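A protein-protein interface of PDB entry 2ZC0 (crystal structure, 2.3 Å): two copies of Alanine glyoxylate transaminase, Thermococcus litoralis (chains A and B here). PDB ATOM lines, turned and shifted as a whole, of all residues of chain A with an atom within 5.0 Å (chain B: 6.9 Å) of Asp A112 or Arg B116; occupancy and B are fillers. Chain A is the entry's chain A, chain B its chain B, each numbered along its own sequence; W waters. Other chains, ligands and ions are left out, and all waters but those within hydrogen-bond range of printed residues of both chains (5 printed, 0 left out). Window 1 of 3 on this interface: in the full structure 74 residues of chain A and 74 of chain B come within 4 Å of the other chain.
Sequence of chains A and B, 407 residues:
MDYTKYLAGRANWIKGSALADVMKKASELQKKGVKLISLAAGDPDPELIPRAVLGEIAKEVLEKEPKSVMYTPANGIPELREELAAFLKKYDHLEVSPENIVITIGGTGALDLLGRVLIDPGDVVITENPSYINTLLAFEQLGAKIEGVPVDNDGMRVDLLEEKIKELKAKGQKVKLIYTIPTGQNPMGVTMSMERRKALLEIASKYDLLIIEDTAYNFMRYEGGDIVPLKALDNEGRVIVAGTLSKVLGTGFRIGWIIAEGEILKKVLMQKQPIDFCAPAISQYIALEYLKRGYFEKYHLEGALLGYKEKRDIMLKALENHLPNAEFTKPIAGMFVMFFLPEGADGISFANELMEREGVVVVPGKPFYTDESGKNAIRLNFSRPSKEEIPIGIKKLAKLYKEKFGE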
ATOM      1  N   ALA A   8      21.348  15.082 -14.517  1.00  0.00           N
ATOM      2  CA  ALA A   8      19.896  15.114 -14.483  1.00  0.00           C
ATOM      3  C   ALA A   8      19.566  14.333 -13.211  1.00  0.00           C
ATOM      4  O   ALA A   8      20.342  13.473 -12.789  1.00  0.00           O
ATOM      5  CB  ALA A   8      19.322  14.417 -15.705  1.00  0.00           C
ATOM      6  N   ARG A  10      17.445  12.039 -12.817  1.00  0.00           N
ATOM      7  CA  ARG A  10      17.358  10.630 -13.173  1.00  0.00           C
ATOM      8  C   ARG A  10      18.710   9.931 -13.319  1.00  0.00           C
ATOM      9  O   ARG A  10      18.756   8.710 -13.407  1.00  0.00           O
ATOM     10  CB  ARG A  10      16.531  10.444 -14.445  1.00  0.00           C
ATOM     11  CG  ARG A  10      16.843  11.415 -15.566  1.00  0.00           C
ATOM     12  CD  ARG A  10      16.147  10.976 -16.850  1.00  0.00           C
ATOM     13  NE  ARG A  10      14.752  10.612 -16.605  1.00  0.00           N
ATOM     14  CZ  ARG A  10      14.141   9.538 -17.114  1.00  0.00           C
ATOM     15  NH1 ARG A  10      14.795   8.700 -17.911  1.00  0.00           N
ATOM     16  NH2 ARG A  10      12.873   9.300 -16.813  1.00  0.00           N
ATOM     17  N   ALA A  11      19.801  10.693 -13.341  1.00  0.00           N
ATOM     18  CA  ALA A  11      21.124  10.099 -13.454  1.00  0.00           C
ATOM     19  C   ALA A  11      21.387   9.331 -12.149  1.00  0.00           C
ATOM     20  O   ALA A  11      22.163   8.383 -12.120  1.00  0.00           O
ATOM     21  CB  ALA A  11      22.199  11.191 -13.663  1.00  0.00           C
ATOM     22  N   THR A 108      20.249  -6.486 -25.652  1.00  0.00           N
ATOM     23  CA  THR A 108      20.340  -5.358 -24.724  1.00  0.00           C
ATOM     24  C   THR A 108      19.619  -4.143 -25.300  1.00  0.00           C
ATOM     25  O   THR A 108      18.764  -3.556 -24.651  1.00  0.00           O
ATOM     26  CB  THR A 108      21.820  -4.953 -24.454  1.00  0.00           C
ATOM     27  OG1 THR A 108      22.534  -6.062 -23.895  1.00  0.00           O
ATOM     28  CG2 THR A 108      21.892  -3.771 -23.480  1.00  0.00           C
ATOM     29  N   GLY A 109      19.979  -3.768 -26.521  1.00  0.00           N
ATOM     30  CA  GLY A 109      19.344  -2.628 -27.162  1.00  0.00           C
ATOM     31  C   GLY A 109      17.851  -2.834 -27.271  1.00  0.00           C
ATOM     32  O   GLY A 109      17.075  -1.922 -27.015  1.00  0.00           O
ATOM     33  N   ALA A 110      17.449  -4.048 -27.638  1.00  0.00           N
ATOM     34  CA  ALA A 110      16.031  -4.388 -27.768  1.00  0.00           C
ATOM     35  C   ALA A 110      15.308  -4.126 -26.453  1.00  0.00           C
ATOM     36  O   ALA A 110      14.234  -3.529 -26.429  1.00  0.00           O
ATOM     37  CB  ALA A 110      15.878  -5.854 -28.170  1.00  0.00           C
ATOM     38  N   LEU A 111      15.910  -4.573 -25.359  1.00  0.00           N
ATOM     39  CA  LEU A 111      15.317  -4.403 -24.035  1.00  0.00           C
ATOM     40  C   LEU A 111      15.295  -2.924 -23.598  1.00  0.00           C
ATOM     41  O   LEU A 111      14.382  -2.502 -22.898  1.00  0.00           O
ATOM     42  CB  LEU A 111      16.085  -5.248 -23.008  1.00  0.00           C
ATOM     43  CG  LEU A 111      15.605  -6.638 -22.522  1.00  0.00           C
ATOM     44  CD1 LEU A 111      14.280  -7.034 -23.136  1.00  0.00           C
ATOM     45  CD2 LEU A 111      16.685  -7.665 -22.822  1.00  0.00           C
ATOM     46  N   ASP A 112      16.298  -2.148 -24.002  1.00  0.00           N
ATOM     47  CA  ASP A 112      16.360  -0.728 -23.658  1.00  0.00           C
ATOM     48  C   ASP A 112      15.307   0.032 -24.483  1.00  0.00           C
ATOM     49  O   ASP A 112      14.575   0.876 -23.960  1.00  0.00           O
ATOM     50  CB  ASP A 112      17.775  -0.192 -23.939  1.00  0.00           C
ATOM     51  CG  ASP A 112      17.885   1.316 -23.756  1.00  0.00           C
ATOM     52  OD1 ASP A 112      17.839   2.027 -24.782  1.00  0.00           O
ATOM     53  OD2 ASP A 112      18.006   1.786 -22.610  1.00  0.00           O
ATOM     54  N   LEU A 113      15.223  -0.289 -25.769  1.00  0.00           N
ATOM     55  CA  LEU A 113      14.235   0.339 -26.633  1.00  0.00           C
ATOM     56  C   LEU A 113      12.822   0.080 -26.081  1.00  0.00           C
ATOM     57  O   LEU A 113      12.010   0.999 -25.990  1.00  0.00           O
ATOM     58  CB  LEU A 113      14.387  -0.195 -28.070  1.00  0.00           C
ATOM     59  CG  LEU A 113      15.083   0.771 -29.052  1.00  0.00           C
ATOM     60  CD1 LEU A 113      16.228   1.465 -28.369  1.00  0.00           C
ATOM     61  CD2 LEU A 113      15.553   0.034 -30.306  1.00  0.00           C
ATOM     62  N   LEU A 114      12.548  -1.161 -25.677  1.00  0.00           N
ATOM     63  CA  LEU A 114      11.247  -1.505 -25.116  1.00  0.00           C
ATOM     64  C   LEU A 114      10.969  -0.788 -23.785  1.00  0.00           C
ATOM     65  O   LEU A 114       9.847  -0.352 -23.530  1.00  0.00           O
ATOM     66  CB  LEU A 114      11.132  -3.024 -24.883  1.00  0.00           C
ATOM     67  CG  LEU A 114      10.513  -3.974 -25.935  1.00  0.00           C
ATOM     68  CD1 LEU A 114       9.820  -3.189 -27.069  1.00  0.00           C
ATOM     69  CD2 LEU A 114      11.587  -4.875 -26.461  1.00  0.00           C
ATOM     70  N   GLY A 115      11.976  -0.688 -22.923  1.00  0.00           N
ATOM     71  CA  GLY A 115      11.760  -0.036 -21.648  1.00  0.00           C
ATOM     72  C   GLY A 115      11.411   1.426 -21.819  1.00  0.00           C
ATOM     73  O   GLY A 115      10.577   1.980 -21.098  1.00  0.00           O
ATOM     74  N   ARG A 116      12.045   2.058 -22.791  1.00  0.00           N
ATOM     75  CA  ARG A 116      11.798   3.465 -23.031  1.00  0.00           C
ATOM     76  C   ARG A 116      10.379   3.751 -23.520  1.00  0.00           C
ATOM     77  O   ARG A 116       9.810   4.786 -23.214  1.00  0.00           O
ATOM     78  CB  ARG A 116      12.838   3.995 -24.009  1.00  0.00           C
ATOM     79  CG  ARG A 116      14.248   3.885 -23.448  1.00  0.00           C
ATOM     80  CD  ARG A 116      15.250   4.527 -24.387  1.00  0.00           C
ATOM     81  NE  ARG A 116      14.745   5.828 -24.816  1.00  0.00           N
ATOM     82  CZ  ARG A 116      15.493   6.820 -25.281  1.00  0.00           C
ATOM     83  NH1 ARG A 116      16.815   6.658 -25.375  1.00  0.00           N
ATOM     84  NH2 ARG A 116      14.901   7.960 -25.645  1.00  0.00           N
ATOM     85  N   ALA A 138      18.914  -1.886 -16.414  1.00  0.00           N
ATOM     86  CA  ALA A 138      18.342  -1.120 -17.515  1.00  0.00           C
ATOM     87  C   ALA A 138      16.973  -0.566 -17.151  1.00  0.00           C
ATOM     88  O   ALA A 138      16.710   0.613 -17.365  1.00  0.00           O
ATOM     89  CB  ALA A 138      18.230  -1.981 -18.779  1.00  0.00           C
ATOM     90  N   GLN A 141      17.143   2.154 -14.188  1.00  0.00           N
ATOM     91  CA  GLN A 141      17.661   3.479 -14.509  1.00  0.00           C
ATOM     92  C   GLN A 141      16.642   4.213 -15.378  1.00  0.00           C
ATOM     93  O   GLN A 141      16.797   5.390 -15.667  1.00  0.00           O
ATOM     94  CB  GLN A 141      19.054   3.435 -15.165  1.00  0.00           C
ATOM     95  CG  GLN A 141      19.200   2.611 -16.395  1.00  0.00           C
ATOM     96  CD  GLN A 141      20.656   2.484 -16.813  1.00  0.00           C
ATOM     97  OE1 GLN A 141      21.561   2.587 -15.985  1.00  0.00           O
ATOM     98  NE2 GLN A 141      20.885   2.252 -18.088  1.00  0.00           N
ATOM     99  N   LEU A 142      15.590   3.502 -15.784  1.00  0.00           N
ATOM    100  CA  LEU A 142      14.512   4.131 -16.538  1.00  0.00           C
ATOM    101  C   LEU A 142      13.442   4.481 -15.510  1.00  0.00           C
ATOM    102  O   LEU A 142      12.360   4.929 -15.856  1.00  0.00           O
ATOM    103  CB  LEU A 142      13.955   3.208 -17.616  1.00  0.00           C
ATOM    104  CG  LEU A 142      14.861   3.122 -18.865  1.00  0.00           C
ATOM    105  CD1 LEU A 142      14.443   1.936 -19.775  1.00  0.00           C
ATOM    106  CD2 LEU A 142      14.751   4.457 -19.644  1.00  0.00           C
ATOM    107  N   ILE A 275      18.347   7.101 -31.579  1.00  0.00           N
ATOM    108  CA  ILE A 275      19.124   6.583 -30.459  1.00  0.00           C
ATOM    109  C   ILE A 275      20.315   5.726 -30.904  1.00  0.00           C
ATOM    110  O   ILE A 275      21.388   5.852 -30.329  1.00  0.00           O
ATOM    111  CB  ILE A 275      18.267   5.843 -29.381  1.00  0.00           C
ATOM    112  CG1 ILE A 275      18.767   4.419 -29.214  1.00  0.00           C
ATOM    113  CG2 ILE A 275      16.798   5.914 -29.702  1.00  0.00           C
ATOM    114  CD1 ILE A 275      18.341   3.825 -27.922  1.00  0.00           C
ATOM    115  N   LEU B 111      25.199  10.976 -28.390  1.00  0.00           N
ATOM    116  CA  LEU B 111      24.260  12.037 -28.050  1.00  0.00           C
ATOM    117  C   LEU B 111      23.121  11.532 -27.158  1.00  0.00           C
ATOM    118  O   LEU B 111      22.685  12.233 -26.245  1.00  0.00           O
ATOM    119  CB  LEU B 111      23.659  12.671 -29.323  1.00  0.00           C
ATOM    120  CG  LEU B 111      24.382  13.743 -30.152  1.00  0.00           C
ATOM    121  CD1 LEU B 111      25.467  14.403 -29.334  1.00  0.00           C
ATOM    122  CD2 LEU B 111      24.947  13.145 -31.405  1.00  0.00           C
ATOM    123  N   ASP B 112      22.627  10.329 -27.436  1.00  0.00           N
ATOM    124  CA  ASP B 112      21.544   9.756 -26.638  1.00  0.00           C
ATOM    125  C   ASP B 112      22.016   9.432 -25.220  1.00  0.00           C
ATOM    126  O   ASP B 112      21.316   9.699 -24.240  1.00  0.00           O
ATOM    127  CB  ASP B 112      20.984   8.500 -27.320  1.00  0.00           C
ATOM    128  CG  ASP B 112      20.028   7.725 -26.425  1.00  0.00           C
ATOM    129  OD1 ASP B 112      20.479   6.728 -25.806  1.00  0.00           O
ATOM    130  OD2 ASP B 112      18.843   8.116 -26.313  1.00  0.00           O
ATOM    131  N   LEU B 113      23.211   8.865 -25.103  1.00  0.00           N
ATOM    132  CA  LEU B 113      23.773   8.547 -23.789  1.00  0.00           C
ATOM    133  C   LEU B 113      23.912   9.823 -22.972  1.00  0.00           C
ATOM    134  O   LEU B 113      23.537   9.861 -21.801  1.00  0.00           O
ATOM    135  CB  LEU B 113      25.141   7.867 -23.954  1.00  0.00           C
ATOM    136  CG  LEU B 113      25.212   6.398 -23.539  1.00  0.00           C
ATOM    137  CD1 LEU B 113      23.853   5.747 -23.714  1.00  0.00           C
ATOM    138  CD2 LEU B 113      26.290   5.667 -24.342  1.00  0.00           C
ATOM    139  N   LEU B 114      24.440  10.881 -23.588  1.00  0.00           N
ATOM    140  CA  LEU B 114      24.600  12.164 -22.872  1.00  0.00           C
ATOM    141  C   LEU B 114      23.257  12.759 -22.478  1.00  0.00           C
ATOM    142  O   LEU B 114      23.110  13.296 -21.388  1.00  0.00           O
ATOM    143  CB  LEU B 114      25.368  13.191 -23.719  1.00  0.00           C
ATOM    144  CG  LEU B 114      26.892  13.409 -23.710  1.00  0.00           C
ATOM    145  CD1 LEU B 114      27.598  12.782 -22.515  1.00  0.00           C
ATOM    146  CD2 LEU B 114      27.439  12.889 -24.996  1.00  0.00           C
ATOM    147  N   GLY B 115      22.275  12.674 -23.366  1.00  0.00           N
ATOM    148  CA  GLY B 115      20.960  13.222 -23.048  1.00  0.00           C
ATOM    149  C   GLY B 115      20.376  12.561 -21.813  1.00  0.00           C
ATOM    150  O   GLY B 115      19.834  13.228 -20.928  1.00  0.00           O
ATOM    151  N   ARG B 116      20.499  11.239 -21.759  1.00  0.00           N
ATOM    152  CA  ARG B 116      19.992  10.444 -20.645  1.00  0.00           C
ATOM    153  C   ARG B 116      20.604  10.795 -19.291  1.00  0.00           C
ATOM    154  O   ARG B 116      19.952  10.683 -18.257  1.00  0.00           O
ATOM    155  CB  ARG B 116      20.216   8.961 -20.923  1.00  0.00           C
ATOM    156  CG  ARG B 116      19.438   8.453 -22.128  1.00  0.00           C
ATOM    157  CD  ARG B 116      19.538   6.951 -22.228  1.00  0.00           C
ATOM    158  NE  ARG B 116      19.138   6.353 -20.960  1.00  0.00           N
ATOM    159  CZ  ARG B 116      18.660   5.125 -20.822  1.00  0.00           C
ATOM    160  NH1 ARG B 116      18.513   4.343 -21.896  1.00  0.00           N
ATOM    161  NH2 ARG B 116      18.334   4.702 -19.607  1.00  0.00           N
ATOM    162  N   VAL B 117      21.852  11.233 -19.304  1.00  0.00           N
ATOM    163  CA  VAL B 117      22.535  11.584 -18.077  1.00  0.00           C
ATOM    164  C   VAL B 117      22.442  13.070 -17.735  1.00  0.00           C
ATOM    165  O   VAL B 117      22.549  13.458 -16.565  1.00  0.00           O
ATOM    166  CB  VAL B 117      24.015  11.158 -18.173  1.00  0.00           C
ATOM    167  CG1 VAL B 117      24.888  12.028 -17.286  1.00  0.00           C
ATOM    168  CG2 VAL B 117      24.148   9.714 -17.748  1.00  0.00           C
ATOM    169  N   LEU B 118      22.218  13.905 -18.742  1.00  0.00           N
ATOM    170  CA  LEU B 118      22.160  15.333 -18.499  1.00  0.00           C
ATOM    171  C   LEU B 118      20.799  15.996 -18.590  1.00  0.00           C
ATOM    172  O   LEU B 118      20.662  17.151 -18.189  1.00  0.00           O
ATOM    173  CB  LEU B 118      23.129  16.042 -19.449  1.00  0.00           C
ATOM    174  CG  LEU B 118      24.578  15.583 -19.341  1.00  0.00           C
ATOM    175  CD1 LEU B 118      25.404  16.280 -20.401  1.00  0.00           C
ATOM    176  CD2 LEU B 118      25.099  15.876 -17.930  1.00  0.00           C
ATOM    177  N   ILE B 119      19.793  15.276 -19.089  1.00  0.00           N
ATOM    178  CA  ILE B 119      18.461  15.864 -19.252  1.00  0.00           C
ATOM    179  C   ILE B 119      17.313  15.373 -18.376  1.00  0.00           C
ATOM    180  O   ILE B 119      16.980  14.191 -18.382  1.00  0.00           O
ATOM    181  CB  ILE B 119      17.979  15.726 -20.720  1.00  0.00           C
ATOM    182  CG1 ILE B 119      18.919  16.478 -21.666  1.00  0.00           C
ATOM    183  CG2 ILE B 119      16.568  16.292 -20.869  1.00  0.00           C
ATOM    184  CD1 ILE B 119      18.768  16.004 -23.100  1.00  0.00           C
ATOM    185  N   ASP B 120      16.705  16.284 -17.623  1.00  0.00           N
ATOM    186  CA  ASP B 120      15.528  15.953 -16.821  1.00  0.00           C
ATOM    187  C   ASP B 120      14.373  16.471 -17.678  1.00  0.00           C
ATOM    188  O   ASP B 120      14.506  17.489 -18.371  1.00  0.00           O
ATOM    189  CB  ASP B 120      15.522  16.675 -15.460  1.00  0.00           C
ATOM    190  CG  ASP B 120      16.368  15.970 -14.399  1.00  0.00           C
ATOM    191  OD1 ASP B 120      16.199  14.745 -14.190  1.00  0.00           O
ATOM    192  OD2 ASP B 120      17.200  16.645 -13.759  1.00  0.00           O
ATOM    193  N   PHE B 139      16.661  14.541 -28.155  1.00  0.00           N
ATOM    194  CA  PHE B 139      16.511  15.280 -26.907  1.00  0.00           C
ATOM    195  C   PHE B 139      15.063  15.478 -26.475  1.00  0.00           C
ATOM    196  O   PHE B 139      14.755  15.412 -25.288  1.00  0.00           O
ATOM    197  CB  PHE B 139      17.205  16.646 -27.020  1.00  0.00           C
ATOM    198  CG  PHE B 139      18.698  16.564 -27.051  1.00  0.00           C
ATOM    199  CD1 PHE B 139      19.347  15.361 -26.759  1.00  0.00           C
ATOM    200  CD2 PHE B 139      19.471  17.695 -27.320  1.00  0.00           C
ATOM    201  CE1 PHE B 139      20.725  15.285 -26.730  1.00  0.00           C
ATOM    202  CE2 PHE B 139      20.860  17.622 -27.290  1.00  0.00           C
ATOM    203  CZ  PHE B 139      21.491  16.405 -26.991  1.00  0.00           C
ATOM    204  N   LEU B 142      13.367  12.722 -24.915  1.00  0.00           N
ATOM    205  CA  LEU B 142      13.875  12.557 -23.554  1.00  0.00           C
ATOM    206  C   LEU B 142      13.205  13.631 -22.697  1.00  0.00           C
ATOM    207  O   LEU B 142      13.560  13.819 -21.549  1.00  0.00           O
ATOM    208  CB  LEU B 142      15.393  12.696 -23.480  1.00  0.00           C
ATOM    209  CG  LEU B 142      16.216  11.494 -23.984  1.00  0.00           C
ATOM    210  CD1 LEU B 142      17.675  11.905 -24.078  1.00  0.00           C
ATOM    211  CD2 LEU B 142      16.059  10.283 -23.050  1.00  0.00           C
ATOM    212  N   GLN B 271      25.867   3.684 -16.932  1.00  0.00           N
ATOM    213  CA  GLN B 271      24.619   3.354 -17.620  1.00  0.00           C
ATOM    214  C   GLN B 271      24.788   2.598 -18.940  1.00  0.00           C
ATOM    215  O   GLN B 271      23.862   1.930 -19.395  1.00  0.00           O
ATOM    216  CB  GLN B 271      23.823   4.632 -17.911  1.00  0.00           C
ATOM    217  CG  GLN B 271      24.386   5.463 -19.097  1.00  0.00           C
ATOM    218  CD  GLN B 271      23.540   6.691 -19.460  1.00  0.00           C
ATOM    219  OE1 GLN B 271      22.408   6.842 -19.023  1.00  0.00           O
ATOM    220  NE2 GLN B 271      24.097   7.558 -20.277  1.00  0.00           N
ATOM    221  N   PRO B 274      24.133  -1.659 -19.715  1.00  0.00           N
ATOM    222  CA  PRO B 274      22.715  -2.017 -19.753  1.00  0.00           C
ATOM    223  C   PRO B 274      21.939  -1.467 -20.963  1.00  0.00           C
ATOM    224  O   PRO B 274      20.791  -1.872 -21.190  1.00  0.00           O
ATOM    225  CB  PRO B 274      22.178  -1.486 -18.416  1.00  0.00           C
ATOM    226  CG  PRO B 274      23.403  -1.429 -17.530  1.00  0.00           C
ATOM    227  CD  PRO B 274      24.451  -0.926 -18.475  1.00  0.00           C
ATOM    228  N   ILE B 275      22.516  -0.550 -21.740  1.00  0.00           N
ATOM    229  CA  ILE B 275      21.760  -0.096 -22.897  1.00  0.00           C
ATOM    230  C   ILE B 275      22.285  -0.616 -24.239  1.00  0.00           C
ATOM    231  O   ILE B 275      21.487  -0.991 -25.095  1.00  0.00           O
ATOM    232  CB  ILE B 275      21.567   1.451 -22.956  1.00  0.00           C
ATOM    233  CG1 ILE B 275      22.303   2.025 -24.150  1.00  0.00           C
ATOM    234  CG2 ILE B 275      21.950   2.102 -21.650  1.00  0.00           C
ATOM    235  CD1 ILE B 275      21.706   3.315 -24.594  1.00  0.00           C
ATOM    236  N   ASP B 276      23.601  -0.648 -24.441  1.00  0.00           N
ATOM    237  CA  ASP B 276      24.122  -1.203 -25.692  1.00  0.00           C
ATOM    238  C   ASP B 276      25.152  -2.310 -25.439  1.00  0.00           C
ATOM    239  O   ASP B 276      25.574  -2.995 -26.366  1.00  0.00           O
ATOM    240  CB  ASP B 276      24.750  -0.120 -26.604  1.00  0.00           C
ATOM    241  CG  ASP B 276      26.106   0.387 -26.113  1.00  0.00           C
ATOM    242  OD1 ASP B 276      26.808  -0.326 -25.363  1.00  0.00           O
ATOM    243  OD2 ASP B 276      26.485   1.516 -26.508  1.00  0.00           O
HETATM  244  O   HOH W   1      18.874  -3.770 -21.675  1.00  0.00           O
HETATM  245  O   HOH W   2      18.244   1.961 -19.273  1.00  0.00           O
HETATM  246  O   HOH W   3      16.346   9.844 -27.392  1.00  0.00           O
HETATM  247  O   HOH W   4      18.880   4.971 -24.497  1.00  0.00           O
HETATM  248  O   HOH W   5      17.885   8.790 -18.123  1.00  0.00           O
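Among the printed residues, pairs that only touch across the chains: Thr A108 with Pro B274 (3.2 Å), Ala A8 with Asp B120 (3.2 Å), Thr A108 with Ile B275 (3.2 Å), Ala A8 with Ile B119 (3.5 Å), Ala A138 with Pro B274 (3.5 Å), Leu A142 with Arg B116 (3.6 Å), Asp A112 with Ile B275 (3.6 Å), Ala A8 with Leu B118 (3.6 Å), Arg A10 with Ile B119 (3.7 Å), Arg A116 with Leu B142 (3.7 Å), Thr A108 with Asp B276 (3.7 Å), Ala A11 with Val B117 (3.7 Å), Gln A141 with Ile B275 (3.7 Å), Gln A141 with Arg B116 (3.8 Å), Ile A275 with Asp B112 (3.9 Å) and Gln A141 with Pro B274 (3.97 Å).
The backbone carbonyl oxygen of Leu B113 lies within hydrogen-bond range of the side-chain amide nitrogen of Gln B271 (2.8 Å).
Of the 16 printed residues of chain A, 11 touch a printed residue of chain B.
Hydrophobic or aromatic side chains of chain A within 4 Å of the printed part of chain B: Ala A8, Ala A11, Ala A138, Leu A142 and Ile A275.
Among the printed residues, 22 pairs touch across the chains.
Among the printed residues, Asp or Glu carboxylates within 4 Å of a Lys or Arg side-chain nitrogen of the other chain: Asp A112 with Arg B116 (2.7 Å) and Arg A116 with Asp B112 (2.7 Å).
Asp A112 touches Arg B116, and with the chains exchanged Arg A116 touches Asp B112.
Asp A112 touches Ile B275, and with the chains exchanged Ile A275 touches Asp B112.
Arg A116 touches Leu B142, and with the chains exchanged Leu A142 touches Arg B116.
Positions printed for both chains: 111, 112, 113, 114, 115, 116, 142 and 275.
Asp A112 touches just these residues of chain B: Arg B116 (2.7 Å) and Ile B275 (3.6 Å).
Arg B116 touches just these residues of chain A: Asp A112, Gln A141 and Leu A142.
Of the printed residues of chain A, Ile B119 touches Ala A8 (3.5 Å) and Arg A10 (3.7 Å).
Printed residues of chain A within 4 Å of Val B117: Ala A8 and Ala A11.
Printed residues of chain B within 4 Å of Leu A142: Arg B116.
Of the printed residues of chain B, Thr A108 touches Pro B274, Ile B275 and Asp B276.
Printed residues of chain A within 4 Å of Leu B142: Arg A116 (3.7 Å).
Leu A113 touches none of the printed residues of chain B.
The nearest residue of chain A that does not touch Arg B116 is Arg A10 (4.1 Å).
Water W4 lies within hydrogen-bond range of NH1 of Arg B116 (2.7 Å), OD1 of Asp B112 (2.7 Å), NH1 of Arg A116 (2.8 Å) and OD1 of Asp A112 (3.1 Å).
Water W1 lies within hydrogen-bond range of the backbone carbonyl oxygen (O) of Pro B274 (2.7 Å) and the backbone carbonyl oxygen (O) of Thr A108 (3.0 Å).
Water W2 lies within hydrogen-bond range of NH2 of Arg B116 (2.8 Å), O of Ala A138 (2.8 Å), NE2 of Gln A141 (2.9 Å) and OD2 of Asp A112 (3.4 Å).
Water W5 lies within hydrogen-bond range of O of Arg B116 and NH1 of Arg A10.
Water W3 lies within hydrogen-bond range of the guanidinium group of Arg A116 (2.9 Å) and the side-chain carboxylate of Asp B112 (3.2 Å).
O of Val B117 lies within hydrogen-bond range of N of Ala A8 (2.9 Å).
The backbone NH (N) of Arg A10 is in hydrogen-bond range of the side-chain carboxylate (OD1) of Asp B120.
N of Gly A109 sits close to O of Ile B275 (3.5 Å).
OD2 of Asp A112 lies within salt-bridge range of NH1 of Arg B116 (2.7 Å).
The side-chain carboxylate (OD2) of Asp B112 lies within salt-bridge range of the guanidinium group (NH1) of Arg A116 (2.7 Å).
The side-chain amide nitrogen of Gln A141 sits at hydrogen-bond distance from the backbone carbonyl oxygen of Gln B271.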
